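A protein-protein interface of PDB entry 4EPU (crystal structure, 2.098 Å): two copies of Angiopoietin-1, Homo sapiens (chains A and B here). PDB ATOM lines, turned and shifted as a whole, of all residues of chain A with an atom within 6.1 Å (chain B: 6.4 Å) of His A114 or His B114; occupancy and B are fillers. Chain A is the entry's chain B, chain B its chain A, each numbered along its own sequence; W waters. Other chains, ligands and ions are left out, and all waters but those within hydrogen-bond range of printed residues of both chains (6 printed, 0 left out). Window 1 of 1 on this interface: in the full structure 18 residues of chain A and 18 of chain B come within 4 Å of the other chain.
Among the printed residues, merely in contact across the chains: Tyr A125 with Tyr B125 (3.3 Å), Ser A88 with Gln B120 (3.7 Å), Gln A120 with Ser B88 (3.7 Å), Arg A112 with Gln B120 (3.8 Å), Gln A120 with Arg B112 (3.8 Å), Tyr A125 with Leu B126 (3.9 Å) and Leu A126 with Tyr B125 (3.95 Å).
The backbone NH (N) of Tyr B125 is in hydrogen-bond range of the backbone carbonyl oxygen (O) of His B114. The backbone NH of Gln B120 lies within hydrogen-bond range of the side-chain amide oxygen of Asn B117, 2.8 Å away. The backbone carbonyl oxygen (O) of Asn B117 is in hydrogen-bond range of the backbone NH (N) of Tyr B122 (3.0 Å). The guanidinium group (NE) of Arg B123 is in hydrogen-bond range of the side-chain hydroxyl (OH) of Tyr B125 (3.1 Å). The backbone NH (N) of Gly A116 lies within hydrogen-bond range of the backbone carbonyl oxygen (O) of Arg A123 (2.9 Å). The guanidinium group of Arg A123 is in hydrogen-bond range of the side-chain hydroxyl of Tyr A125, at 3.1 Å.
Water W6 lies within hydrogen-bond range of the side-chain hydroxyl of Tyr B125 (2.6 Å), the backbone carbonyl oxygen of Tyr A125 (3.0 Å), the backbone carbonyl oxygen of Arg A112 (3.4 Å) and the backbone NH of Phe A113 (3.5 Å). Water W1 lies within hydrogen-bond range of the side-chain hydroxyl (OH) of Tyr A125 (2.7 Å), the backbone carbonyl oxygen (O) of Tyr B125 (3.2 Å) and the backbone NH (N) of His B114 (3.4 Å). Water W4 lies within hydrogen-bond range of OG of Ser B88 (2.8 Å), NE2 of Gln A120 (2.8 Å) and O of Ile B115 (3.1 Å). Water W2 lies within hydrogen-bond range of OG of Ser A88 (2.9 Å), NE2 of Gln B120 (2.9 Å) and O of Ile A115 (3.0 Å). Water W3 bridges the side-chain hydroxyl (OG) of Ser A88 and the side-chain amide nitrogen (ND2) of Asn B117. Water W5 bridges the side-chain hydroxyl (OG) of Ser B88 (3.1 Å) and the side-chain amide nitrogen (ND2) of Asn A117 (3.4 Å).
Of the printed residues of chain B, Ser A88 touches Asn B117 and Gln B120. Of the printed residues of chain B, Arg A112 touches Gln B120 (3.8 Å) and Arg B123 (3.3 Å). Of the printed residues of chain B, His A114 touches His B114 (3.4 Å) and Gln B120 (3.4 Å). Ile A115 touches none of the printed residues of chain B. Of the printed residues of chain B, Gln A120 touches Thr B87 (2.8 Å), Ser B88 (3.7 Å), Arg B112 (3.8 Å) and His B114 (3.4 Å). Of the printed residues of chain A, Arg B123 touches Arg A112. Of the printed residues of chain A, Leu B126 touches Tyr A125 (3.9 Å). The nearest printed residue of chain B that does not touch His A114 is Gly B116 (4.3 Å).
The backbone carbonyl oxygen (O) of Thr B87 is in hydrogen-bond range of the side-chain amide nitrogen (NE2) of Gln A120 (2.8 Å). The backbone carbonyl oxygen of Ser B88 is in hydrogen-bond range of the side-chain amide nitrogen of Asn A117, at 2.8 Å. NE2 of His A114 lies within hydrogen-bond range of NE2 of His B114 (3.4 Å). A ring nitrogen (ND1) of His B114 lies within hydrogen-bond range of the side-chain amide nitrogen (NE2) of Gln A120, 3.4 Å away. The side-chain amide nitrogen (ND2) of Asn B117 sits at hydrogen-bond distance from the backbone carbonyl oxygen (O) of Ser A88. O of Thr A87 is in hydrogen-bond range of NE2 of Gln B120, 2.8 Å away. NE2 of Gln B120 sits at hydrogen-bond distance from ND1 of His A114, 3.4 Å away. The guanidinium group of Arg A112 sits close to the guanidinium group of Arg B123 (3.3 Å). NH1 of Arg B112 sits close to NH1 of Arg A123 (3.3 Å).
Thr A87 touches Gln B120, and with the chains exchanged Gln A120 touches Thr B87. Arg A112 touches Arg B123, and with the chains exchanged Arg A123 touches Arg B112. Tyr B125 touches its own counterpart, Tyr A125. Tyr A125 touches Leu B126, and with the chains exchanged Leu A126 touches Tyr B125. 15 positions are printed for both chains. Of the 16 pairs that touch across the chains among the printed residues, 16 have their exchanged pair printed and touching as well.
Hydrophobic or aromatic side chains of chain A that line the printed part of chain B: His A114 and Tyr A125. Printed residues of chain B that touch a printed residue of chain A: Thr B87, Ser B88, Arg B112, His B114, Asn B117, Gln B120, Arg B123, Tyr B125 and Leu B126. Among the printed residues, 16 pairs touch across the chains.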
ATOM      1  N   THR A  87     -12.317 -26.536  10.028  1.00  0.00           N
ATOM      2  CA  THR A  87     -11.624 -25.707  11.014  1.00  0.00           C
ATOM      3  C   THR A  87     -10.366 -26.382  11.546  1.00  0.00           C
ATOM      4  O   THR A  87      -9.595 -25.779  12.284  1.00  0.00           O
ATOM      5  CB  THR A  87     -12.546 -25.249  12.179  1.00  0.00           C
ATOM      6  OG1 THR A  87     -13.049 -26.385  12.889  1.00  0.00           O
ATOM      7  CG2 THR A  87     -13.705 -24.442  11.636  1.00  0.00           C
ATOM      8  N   SER A  88     -10.155 -27.629  11.152  1.00  0.00           N
ATOM      9  CA  SER A  88      -8.929 -28.336  11.483  1.00  0.00           C
ATOM     10  C   SER A  88      -7.802 -28.077  10.478  1.00  0.00           C
ATOM     11  O   SER A  88      -6.651 -28.395  10.748  1.00  0.00           O
ATOM     12  CB  SER A  88      -9.194 -29.840  11.569  1.00  0.00           C
ATOM     13  OG  SER A  88      -9.835 -30.170  12.782  1.00  0.00           O
ATOM     14  N   TYR A  92      -9.375 -20.475  11.789  1.00  0.00           N
ATOM     15  CA  TYR A  92     -10.541 -19.760  11.270  1.00  0.00           C
ATOM     16  C   TYR A  92     -11.100 -18.749  12.256  1.00  0.00           C
ATOM     17  O   TYR A  92     -10.941 -18.882  13.464  1.00  0.00           O
ATOM     18  CB  TYR A  92     -11.654 -20.744  10.859  1.00  0.00           C
ATOM     19  CG  TYR A  92     -11.347 -21.497   9.580  1.00  0.00           C
ATOM     20  CD1 TYR A  92     -10.479 -22.583   9.582  1.00  0.00           C
ATOM     21  CD2 TYR A  92     -11.910 -21.108   8.373  1.00  0.00           C
ATOM     22  CE1 TYR A  92     -10.183 -23.266   8.412  1.00  0.00           C
ATOM     23  CE2 TYR A  92     -11.623 -21.786   7.198  1.00  0.00           C
ATOM     24  CZ  TYR A  92     -10.758 -22.863   7.223  1.00  0.00           C
ATOM     25  OH  TYR A  92     -10.469 -23.537   6.059  1.00  0.00           O
ATOM     26  N   ARG A 112     -10.900 -16.226  16.934  1.00  0.00           N
ATOM     27  CA  ARG A 112     -10.497 -17.627  16.793  1.00  0.00           C
ATOM     28  C   ARG A 112     -11.660 -18.576  17.066  1.00  0.00           C
ATOM     29  O   ARG A 112     -12.395 -18.427  18.044  1.00  0.00           O
ATOM     30  CB  ARG A 112      -9.306 -17.975  17.700  1.00  0.00           C
ATOM     31  CG  ARG A 112      -7.932 -17.523  17.180  1.00  0.00           C
ATOM     32  CD  ARG A 112      -7.546 -18.206  15.847  1.00  0.00           C
ATOM     33  NE  ARG A 112      -7.191 -19.623  15.978  1.00  0.00           N
ATOM     34  CZ  ARG A 112      -6.012 -20.060  16.418  1.00  0.00           C
ATOM     35  NH1 ARG A 112      -5.073 -19.191  16.785  1.00  0.00           N
ATOM     36  NH2 ARG A 112      -5.770 -21.366  16.501  1.00  0.00           N
ATOM     37  N   PHE A 113     -11.809 -19.568  16.204  1.00  0.00           N
ATOM     38  CA  PHE A 113     -12.892 -20.518  16.354  1.00  0.00           C
ATOM     39  C   PHE A 113     -12.399 -21.902  16.033  1.00  0.00           C
ATOM     40  O   PHE A 113     -11.820 -22.123  14.980  1.00  0.00           O
ATOM     41  CB  PHE A 113     -14.039 -20.152  15.399  1.00  0.00           C
ATOM     42  CG  PHE A 113     -15.041 -21.278  15.152  1.00  0.00           C
ATOM     43  CD1 PHE A 113     -15.909 -21.701  16.145  1.00  0.00           C
ATOM     44  CD2 PHE A 113     -15.124 -21.888  13.912  1.00  0.00           C
ATOM     45  CE1 PHE A 113     -16.835 -22.725  15.915  1.00  0.00           C
ATOM     46  CE2 PHE A 113     -16.051 -22.905  13.675  1.00  0.00           C
ATOM     47  CZ  PHE A 113     -16.906 -23.322  14.676  1.00  0.00           C
ATOM     48  N   HIS A 114     -12.643 -22.847  16.928  1.00  0.00           N
ATOM     49  CA  HIS A 114     -12.749 -24.219  16.451  1.00  0.00           C
ATOM     50  C   HIS A 114     -13.565 -25.088  17.391  1.00  0.00           C
ATOM     51  O   HIS A 114     -14.045 -24.627  18.425  1.00  0.00           O
ATOM     52  CB  HIS A 114     -11.381 -24.838  16.098  1.00  0.00           C
ATOM     53  CG  HIS A 114     -10.697 -25.524  17.241  1.00  0.00           C
ATOM     54  ND1 HIS A 114      -9.438 -25.171  17.671  1.00  0.00           N
ATOM     55  CD2 HIS A 114     -11.087 -26.551  18.031  1.00  0.00           C
ATOM     56  CE1 HIS A 114      -9.087 -25.950  18.677  1.00  0.00           C
ATOM     57  NE2 HIS A 114     -10.069 -26.794  18.916  1.00  0.00           N
ATOM     58  N   ILE A 115     -13.746 -26.337  16.984  1.00  0.00           N
ATOM     59  CA  ILE A 115     -14.465 -27.302  17.783  1.00  0.00           C
ATOM     60  C   ILE A 115     -13.626 -28.552  17.802  1.00  0.00           C
ATOM     61  O   ILE A 115     -12.832 -28.785  16.890  1.00  0.00           O
ATOM     62  CB  ILE A 115     -15.863 -27.603  17.197  1.00  0.00           C
ATOM     63  CG1 ILE A 115     -15.757 -28.225  15.797  1.00  0.00           C
ATOM     64  CG2 ILE A 115     -16.689 -26.333  17.163  1.00  0.00           C
ATOM     65  CD1 ILE A 115     -17.115 -28.606  15.159  1.00  0.00           C
ATOM     66  N   GLY A 116     -13.791 -29.344  18.853  1.00  0.00           N
ATOM     67  CA  GLY A 116     -13.119 -30.623  18.968  1.00  0.00           C
ATOM     68  C   GLY A 116     -13.708 -31.628  18.000  1.00  0.00           C
ATOM     69  O   GLY A 116     -14.665 -31.317  17.285  1.00  0.00           O
ATOM     70  N   ASN A 117     -13.128 -32.823  17.964  1.00  0.00           N
ATOM     71  CA  ASN A 117     -13.635 -33.898  17.130  1.00  0.00           C
ATOM     72  C   ASN A 117     -14.864 -34.538  17.777  1.00  0.00           C
ATOM     73  O   ASN A 117     -15.278 -34.141  18.875  1.00  0.00           O
ATOM     74  CB  ASN A 117     -12.543 -34.948  16.877  1.00  0.00           C
ATOM     75  CG  ASN A 117     -12.042 -35.599  18.154  1.00  0.00           C
ATOM     76  OD1 ASN A 117     -12.757 -35.686  19.148  1.00  0.00           O
ATOM     77  ND2 ASN A 117     -10.802 -36.064  18.128  1.00  0.00           N
ATOM     78  N   GLN A 120     -14.643 -35.625  21.208  1.00  0.00           N
ATOM     79  CA  GLN A 120     -14.668 -34.508  22.146  1.00  0.00           C
ATOM     80  C   GLN A 120     -16.032 -33.809  22.121  1.00  0.00           C
ATOM     81  O   GLN A 120     -16.163 -32.678  22.577  1.00  0.00           O
ATOM     82  CB  GLN A 120     -13.534 -33.530  21.843  1.00  0.00           C
ATOM     83  CG  GLN A 120     -12.129 -34.122  22.063  1.00  0.00           C
ATOM     84  CD  GLN A 120     -11.043 -33.359  21.328  1.00  0.00           C
ATOM     85  OE1 GLN A 120     -11.292 -32.733  20.299  1.00  0.00           O
ATOM     86  NE2 GLN A 120      -9.828 -33.411  21.854  1.00  0.00           N
ATOM     87  N   TYR A 122     -17.576 -32.444  19.811  1.00  0.00           N
ATOM     88  CA  TYR A 122     -17.532 -31.204  19.036  1.00  0.00           C
ATOM     89  C   TYR A 122     -17.511 -29.956  19.930  1.00  0.00           C
ATOM     90  O   TYR A 122     -18.120 -28.932  19.621  1.00  0.00           O
ATOM     91  CB  TYR A 122     -18.686 -31.162  18.041  1.00  0.00           C
ATOM     92  CG  TYR A 122     -18.650 -32.284  17.014  1.00  0.00           C
ATOM     93  CD1 TYR A 122     -17.606 -32.380  16.092  1.00  0.00           C
ATOM     94  CD2 TYR A 122     -19.668 -33.235  16.957  1.00  0.00           C
ATOM     95  CE1 TYR A 122     -17.570 -33.410  15.136  1.00  0.00           C
ATOM     96  CE2 TYR A 122     -19.652 -34.258  16.015  1.00  0.00           C
ATOM     97  CZ  TYR A 122     -18.601 -34.342  15.106  1.00  0.00           C
ATOM     98  OH  TYR A 122     -18.592 -35.358  14.171  1.00  0.00           O
ATOM     99  N   ARG A 123     -16.777 -30.048  21.031  1.00  0.00           N
ATOM    100  CA  ARG A 123     -16.696 -28.963  21.996  1.00  0.00           C
ATOM    101  C   ARG A 123     -16.229 -27.654  21.371  1.00  0.00           C
ATOM    102  O   ARG A 123     -15.298 -27.618  20.570  1.00  0.00           O
ATOM    103  CB  ARG A 123     -15.766 -29.362  23.130  1.00  0.00           C
ATOM    104  CG  ARG A 123     -15.637 -28.353  24.266  1.00  0.00           C
ATOM    105  CD  ARG A 123     -15.399 -29.169  25.501  1.00  0.00           C
ATOM    106  NE  ARG A 123     -15.130 -28.413  26.700  1.00  0.00           N
ATOM    107  CZ  ARG A 123     -15.918 -28.414  27.765  1.00  0.00           C
ATOM    108  NH1 ARG A 123     -17.044 -29.111  27.765  1.00  0.00           N
ATOM    109  NH2 ARG A 123     -15.573 -27.711  28.825  1.00  0.00           N
ATOM    110  N   LEU A 124     -16.885 -26.573  21.762  1.00  0.00           N
ATOM    111  CA  LEU A 124     -16.647 -25.284  21.158  1.00  0.00           C
ATOM    112  C   LEU A 124     -15.598 -24.501  21.941  1.00  0.00           C
ATOM    113  O   LEU A 124     -15.643 -24.463  23.156  1.00  0.00           O
ATOM    114  CB  LEU A 124     -17.965 -24.505  21.104  1.00  0.00           C
ATOM    115  CG  LEU A 124     -17.899 -23.041  20.681  1.00  0.00           C
ATOM    116  CD1 LEU A 124     -17.518 -22.943  19.219  1.00  0.00           C
ATOM    117  CD2 LEU A 124     -19.241 -22.387  20.919  1.00  0.00           C
ATOM    118  N   TYR A 125     -14.596 -23.937  21.279  1.00  0.00           N
ATOM    119  CA  TYR A 125     -13.758 -22.941  21.963  1.00  0.00           C
ATOM    120  C   TYR A 125     -13.555 -21.730  21.057  1.00  0.00           C
ATOM    121  O   TYR A 125     -13.191 -21.856  19.890  1.00  0.00           O
ATOM    122  CB  TYR A 125     -12.410 -23.504  22.480  1.00  0.00           C
ATOM    123  CG  TYR A 125     -12.467 -24.329  23.770  1.00  0.00           C
ATOM    124  CD1 TYR A 125     -12.512 -23.715  25.031  1.00  0.00           C
ATOM    125  CD2 TYR A 125     -12.443 -25.725  23.722  1.00  0.00           C
ATOM    126  CE1 TYR A 125     -12.556 -24.485  26.209  1.00  0.00           C
ATOM    127  CE2 TYR A 125     -12.480 -26.497  24.890  1.00  0.00           C
ATOM    128  CZ  TYR A 125     -12.533 -25.881  26.128  1.00  0.00           C
ATOM    129  OH  TYR A 125     -12.584 -26.671  27.273  1.00  0.00           O
ATOM    130  N   LEU A 126     -13.826 -20.566  21.623  1.00  0.00           N
ATOM    131  CA  LEU A 126     -13.761 -19.281  20.945  1.00  0.00           C
ATOM    132  C   LEU A 126     -12.868 -18.320  21.711  1.00  0.00           C
ATOM    133  O   LEU A 126     -12.631 -18.492  22.905  1.00  0.00           O
ATOM    134  CB  LEU A 126     -15.154 -18.650  20.876  1.00  0.00           C
ATOM    135  CG  LEU A 126     -16.208 -19.383  20.043  1.00  0.00           C
ATOM    136  CD1 LEU A 126     -17.601 -18.862  20.378  1.00  0.00           C
ATOM    137  CD2 LEU A 126     -15.889 -19.232  18.546  1.00  0.00           C
ATOM    138  N   PHE B  84      -1.349 -34.122  21.505  1.00  0.00           N
ATOM    139  CA  PHE B  84      -2.519 -33.943  20.670  1.00  0.00           C
ATOM    140  C   PHE B  84      -3.204 -35.271  20.337  1.00  0.00           C
ATOM    141  O   PHE B  84      -4.424 -35.378  20.415  1.00  0.00           O
ATOM    142  CB  PHE B  84      -2.147 -33.227  19.380  1.00  0.00           C
ATOM    143  CG  PHE B  84      -3.208 -33.340  18.318  1.00  0.00           C
ATOM    144  CD1 PHE B  84      -4.388 -32.611  18.417  1.00  0.00           C
ATOM    145  CD2 PHE B  84      -3.035 -34.187  17.234  1.00  0.00           C
ATOM    146  CE1 PHE B  84      -5.372 -32.714  17.450  1.00  0.00           C
ATOM    147  CE2 PHE B  84      -4.018 -34.300  16.255  1.00  0.00           C
ATOM    148  CZ  PHE B  84      -5.185 -33.560  16.362  1.00  0.00           C
ATOM    149  N   THR B  87      -4.943 -36.709  23.520  1.00  0.00           N
ATOM    150  CA  THR B  87      -6.095 -35.938  23.987  1.00  0.00           C
ATOM    151  C   THR B  87      -7.190 -35.841  22.934  1.00  0.00           C
ATOM    152  O   THR B  87      -8.274 -35.342  23.206  1.00  0.00           O
ATOM    153  CB  THR B  87      -5.709 -34.524  24.515  1.00  0.00           C
ATOM    154  OG1 THR B  87      -5.102 -33.752  23.471  1.00  0.00           O
ATOM    155  CG2 THR B  87      -4.752 -34.646  25.681  1.00  0.00           C
ATOM    156  N   SER B  88      -6.905 -36.334  21.740  1.00  0.00           N
ATOM    157  CA  SER B  88      -7.908 -36.411  20.690  1.00  0.00           C
ATOM    158  C   SER B  88      -8.741 -37.695  20.764  1.00  0.00           C
ATOM    159  O   SER B  88      -9.777 -37.796  20.113  1.00  0.00           O
ATOM    160  CB  SER B  88      -7.241 -36.326  19.317  1.00  0.00           C
ATOM    161  OG  SER B  88      -6.881 -34.996  19.012  1.00  0.00           O
ATOM    162  N   TYR B  92      -9.940 -35.609  28.267  1.00  0.00           N
ATOM    163  CA  TYR B  92      -8.936 -35.724  29.326  1.00  0.00           C
ATOM    164  C   TYR B  92      -8.997 -34.571  30.315  1.00  0.00           C
ATOM    165  O   TYR B  92      -9.433 -33.472  29.991  1.00  0.00           O
ATOM    166  CB  TYR B  92      -7.512 -35.825  28.737  1.00  0.00           C
ATOM    167  CG  TYR B  92      -7.220 -37.175  28.110  1.00  0.00           C
ATOM    168  CD1 TYR B  92      -7.697 -37.490  26.843  1.00  0.00           C
ATOM    169  CD2 TYR B  92      -6.477 -38.135  28.794  1.00  0.00           C
ATOM    170  CE1 TYR B  92      -7.448 -38.729  26.273  1.00  0.00           C
ATOM    171  CE2 TYR B  92      -6.221 -39.373  28.234  1.00  0.00           C
ATOM    172  CZ  TYR B  92      -6.710 -39.665  26.973  1.00  0.00           C
ATOM    173  OH  TYR B  92      -6.460 -40.894  26.414  1.00  0.00           O
ATOM    174  N   ARG B 112     -11.187 -30.044  32.037  1.00  0.00           N
ATOM    175  CA  ARG B 112     -11.099 -30.362  30.611  1.00  0.00           C
ATOM    176  C   ARG B 112      -9.821 -29.805  29.988  1.00  0.00           C
ATOM    177  O   ARG B 112      -9.440 -28.655  30.205  1.00  0.00           O
ATOM    178  CB  ARG B 112     -12.333 -29.868  29.840  1.00  0.00           C
ATOM    179  CG  ARG B 112     -13.584 -30.759  29.965  1.00  0.00           C
ATOM    180  CD  ARG B 112     -13.372 -32.178  29.386  1.00  0.00           C
ATOM    181  NE  ARG B 112     -13.310 -32.227  27.922  1.00  0.00           N
ATOM    182  CZ  ARG B 112     -14.377 -32.175  27.124  1.00  0.00           C
ATOM    183  NH1 ARG B 112     -15.598 -32.056  27.645  1.00  0.00           N
ATOM    184  NH2 ARG B 112     -14.229 -32.231  25.803  1.00  0.00           N
ATOM    185  N   PHE B 113      -9.154 -30.630  29.202  1.00  0.00           N
ATOM    186  CA  PHE B 113      -7.922 -30.206  28.566  1.00  0.00           C
ATOM    187  C   PHE B 113      -7.883 -30.724  27.155  1.00  0.00           C
ATOM    188  O   PHE B 113      -8.062 -31.916  26.928  1.00  0.00           O
ATOM    189  CB  PHE B 113      -6.724 -30.767  29.348  1.00  0.00           C
ATOM    190  CG  PHE B 113      -5.409 -30.762  28.581  1.00  0.00           C
ATOM    191  CD1 PHE B 113      -4.752 -29.579  28.288  1.00  0.00           C
ATOM    192  CD2 PHE B 113      -4.825 -31.949  28.176  1.00  0.00           C
ATOM    193  CE1 PHE B 113      -3.539 -29.570  27.592  1.00  0.00           C
ATOM    194  CE2 PHE B 113      -3.608 -31.949  27.488  1.00  0.00           C
ATOM    195  CZ  PHE B 113      -2.966 -30.753  27.198  1.00  0.00           C
ATOM    196  N   HIS B 114      -7.628 -29.844  26.197  1.00  0.00           N
ATOM    197  CA  HIS B 114      -6.987 -30.334  24.985  1.00  0.00           C
ATOM    198  C   HIS B 114      -6.235 -29.238  24.250  1.00  0.00           C
ATOM    199  O   HIS B 114      -6.208 -28.083  24.676  1.00  0.00           O
ATOM    200  CB  HIS B 114      -7.950 -31.116  24.069  1.00  0.00           C
ATOM    201  CG  HIS B 114      -8.686 -30.267  23.079  1.00  0.00           C
ATOM    202  ND1 HIS B 114     -10.059 -30.217  23.017  1.00  0.00           N
ATOM    203  CD2 HIS B 114      -8.239 -29.444  22.100  1.00  0.00           C
ATOM    204  CE1 HIS B 114     -10.424 -29.402  22.044  1.00  0.00           C
ATOM    205  NE2 HIS B 114      -9.337 -28.918  21.476  1.00  0.00           N
ATOM    206  N   ILE B 115      -5.593 -29.633  23.162  1.00  0.00           N
ATOM    207  CA  ILE B 115      -4.859 -28.710  22.332  1.00  0.00           C
ATOM    208  C   ILE B 115      -5.249 -29.003  20.908  1.00  0.00           C
ATOM    209  O   ILE B 115      -5.648 -30.124  20.589  1.00  0.00           O
ATOM    210  CB  ILE B 115      -3.322 -28.870  22.506  1.00  0.00           C
ATOM    211  CG1 ILE B 115      -2.862 -30.269  22.077  1.00  0.00           C
ATOM    212  CG2 ILE B 115      -2.937 -28.594  23.943  1.00  0.00           C
ATOM    213  CD1 ILE B 115      -1.348 -30.493  22.148  1.00  0.00           C
ATOM    214  N   GLY B 116      -5.146 -27.988  20.059  1.00  0.00           N
ATOM    215  CA  GLY B 116      -5.410 -28.146  18.643  1.00  0.00           C
ATOM    216  C   GLY B 116      -4.307 -28.941  17.974  1.00  0.00           C
ATOM    217  O   GLY B 116      -3.331 -29.331  18.621  1.00  0.00           O
ATOM    218  N   ASN B 117      -4.472 -29.199  16.680  1.00  0.00           N
ATOM    219  CA  ASN B 117      -3.463 -29.895  15.905  1.00  0.00           C
ATOM    220  C   ASN B 117      -2.323 -28.945  15.537  1.00  0.00           C
ATOM    221  O   ASN B 117      -2.366 -27.751  15.863  1.00  0.00           O
ATOM    222  CB  ASN B 117      -4.084 -30.512  14.648  1.00  0.00           C
ATOM    223  CG  ASN B 117      -4.693 -29.476  13.724  1.00  0.00           C
ATOM    224  OD1 ASN B 117      -4.276 -28.320  13.696  1.00  0.00           O
ATOM    225  ND2 ASN B 117      -5.690 -29.889  12.957  1.00  0.00           N
ATOM    226  N   GLN B 120      -3.133 -25.796  13.999  1.00  0.00           N
ATOM    227  CA  GLN B 120      -3.700 -24.841  14.932  1.00  0.00           C
ATOM    228  C   GLN B 120      -2.653 -24.419  15.970  1.00  0.00           C
ATOM    229  O   GLN B 120      -2.995 -23.880  17.021  1.00  0.00           O
ATOM    230  CB  GLN B 120      -4.945 -25.430  15.597  1.00  0.00           C
ATOM    231  CG  GLN B 120      -6.113 -25.664  14.621  1.00  0.00           C
ATOM    232  CD  GLN B 120      -7.135 -26.647  15.153  1.00  0.00           C
ATOM    233  OE1 GLN B 120      -6.816 -27.531  15.949  1.00  0.00           O
ATOM    234  NE2 GLN B 120      -8.374 -26.504  14.704  1.00  0.00           N
ATOM    235  N   TYR B 122      -1.013 -26.106  18.005  1.00  0.00           N
ATOM    236  CA  TYR B 122      -1.213 -26.797  19.279  1.00  0.00           C
ATOM    237  C   TYR B 122      -1.859 -25.907  20.346  1.00  0.00           C
ATOM    238  O   TYR B 122      -1.520 -25.979  21.526  1.00  0.00           O
ATOM    239  CB  TYR B 122       0.100 -27.400  19.771  1.00  0.00           C
ATOM    240  CG  TYR B 122       0.677 -28.452  18.832  1.00  0.00           C
ATOM    241  CD1 TYR B 122      -0.002 -29.645  18.582  1.00  0.00           C
ATOM    242  CD2 TYR B 122       1.896 -28.247  18.195  1.00  0.00           C
ATOM    243  CE1 TYR B 122       0.530 -30.616  17.718  1.00  0.00           C
ATOM    244  CE2 TYR B 122       2.439 -29.200  17.341  1.00  0.00           C
ATOM    245  CZ  TYR B 122       1.754 -30.381  17.107  1.00  0.00           C
ATOM    246  OH  TYR B 122       2.300 -31.319  16.258  1.00  0.00           O
ATOM    247  N   ARG B 123      -2.821 -25.098  19.918  1.00  0.00           N
ATOM    248  CA  ARG B 123      -3.462 -24.130  20.793  1.00  0.00           C
ATOM    249  C   ARG B 123      -4.116 -24.783  22.001  1.00  0.00           C
ATOM    250  O   ARG B 123      -4.774 -25.813  21.898  1.00  0.00           O
ATOM    251  CB  ARG B 123      -4.492 -23.336  20.007  1.00  0.00           C
ATOM    252  CG  ARG B 123      -5.208 -22.243  20.785  1.00  0.00           C
ATOM    253  CD  ARG B 123      -5.532 -21.182  19.773  1.00  0.00           C
ATOM    254  NE  ARG B 123      -6.325 -20.080  20.262  1.00  0.00           N
ATOM    255  CZ  ARG B 123      -5.891 -18.828  20.323  1.00  0.00           C
ATOM    256  NH1 ARG B 123      -4.654 -18.532  19.960  1.00  0.00           N
ATOM    257  NH2 ARG B 123      -6.699 -17.881  20.762  1.00  0.00           N
ATOM    258  N   LEU B 124      -3.934 -24.162  23.155  1.00  0.00           N
ATOM    259  CA  LEU B 124      -4.370 -24.747  24.401  1.00  0.00           C
ATOM    260  C   LEU B 124      -5.784 -24.282  24.759  1.00  0.00           C
ATOM    261  O   LEU B 124      -6.094 -23.109  24.654  1.00  0.00           O
ATOM    262  CB  LEU B 124      -3.381 -24.363  25.511  1.00  0.00           C
ATOM    263  CG  LEU B 124      -3.758 -24.720  26.943  1.00  0.00           C
ATOM    264  CD1 LEU B 124      -3.725 -26.219  27.124  1.00  0.00           C
ATOM    265  CD2 LEU B 124      -2.789 -24.047  27.908  1.00  0.00           C
ATOM    266  N   TYR B 125      -6.683 -25.187  25.114  1.00  0.00           N
ATOM    267  CA  TYR B 125      -7.935 -24.735  25.738  1.00  0.00           C
ATOM    268  C   TYR B 125      -8.241 -25.601  26.959  1.00  0.00           C
ATOM    269  O   TYR B 125      -8.216 -26.826  26.901  1.00  0.00           O
ATOM    270  CB  TYR B 125      -9.135 -24.673  24.760  1.00  0.00           C
ATOM    271  CG  TYR B 125      -9.178 -23.467  23.814  1.00  0.00           C
ATOM    272  CD1 TYR B 125      -9.670 -22.230  24.235  1.00  0.00           C
ATOM    273  CD2 TYR B 125      -8.762 -23.581  22.489  1.00  0.00           C
ATOM    274  CE1 TYR B 125      -9.716 -21.126  23.359  1.00  0.00           C
ATOM    275  CE2 TYR B 125      -8.811 -22.490  21.610  1.00  0.00           C
ATOM    276  CZ  TYR B 125      -9.290 -21.267  22.043  1.00  0.00           C
ATOM    277  OH  TYR B 125      -9.315 -20.187  21.165  1.00  0.00           O
ATOM    278  N   LEU B 126      -8.496 -24.921  28.065  1.00  0.00           N
ATOM    279  CA  LEU B 126      -8.749 -25.522  29.363  1.00  0.00           C
ATOM    280  C   LEU B 126     -10.061 -25.016  29.940  1.00  0.00           C
ATOM    281  O   LEU B 126     -10.549 -23.954  29.562  1.00  0.00           O
ATOM    282  CB  LEU B 126      -7.637 -25.139  30.347  1.00  0.00           C
ATOM    283  CG  LEU B 126      -6.229 -25.655  30.053  1.00  0.00           C
ATOM    284  CD1 LEU B 126      -5.213 -24.887  30.884  1.00  0.00           C
ATOM    285  CD2 LEU B 126      -6.138 -27.178  30.295  1.00  0.00           C
HETATM  286  O   HOH W   1     -10.809 -28.604  26.521  1.00  0.00           O
HETATM  287  O   HOH W   2     -10.547 -28.445  14.938  1.00  0.00           O
HETATM  288  O   HOH W   3      -7.980 -31.982  14.340  1.00  0.00           O
HETATM  289  O   HOH W   4      -7.444 -32.677  20.499  1.00  0.00           O
HETATM  290  O   HOH W   5      -8.491 -34.143  16.521  1.00  0.00           O
HETATM  291  O   HOH W   6     -10.463 -21.067  19.023  1.00  0.00           O
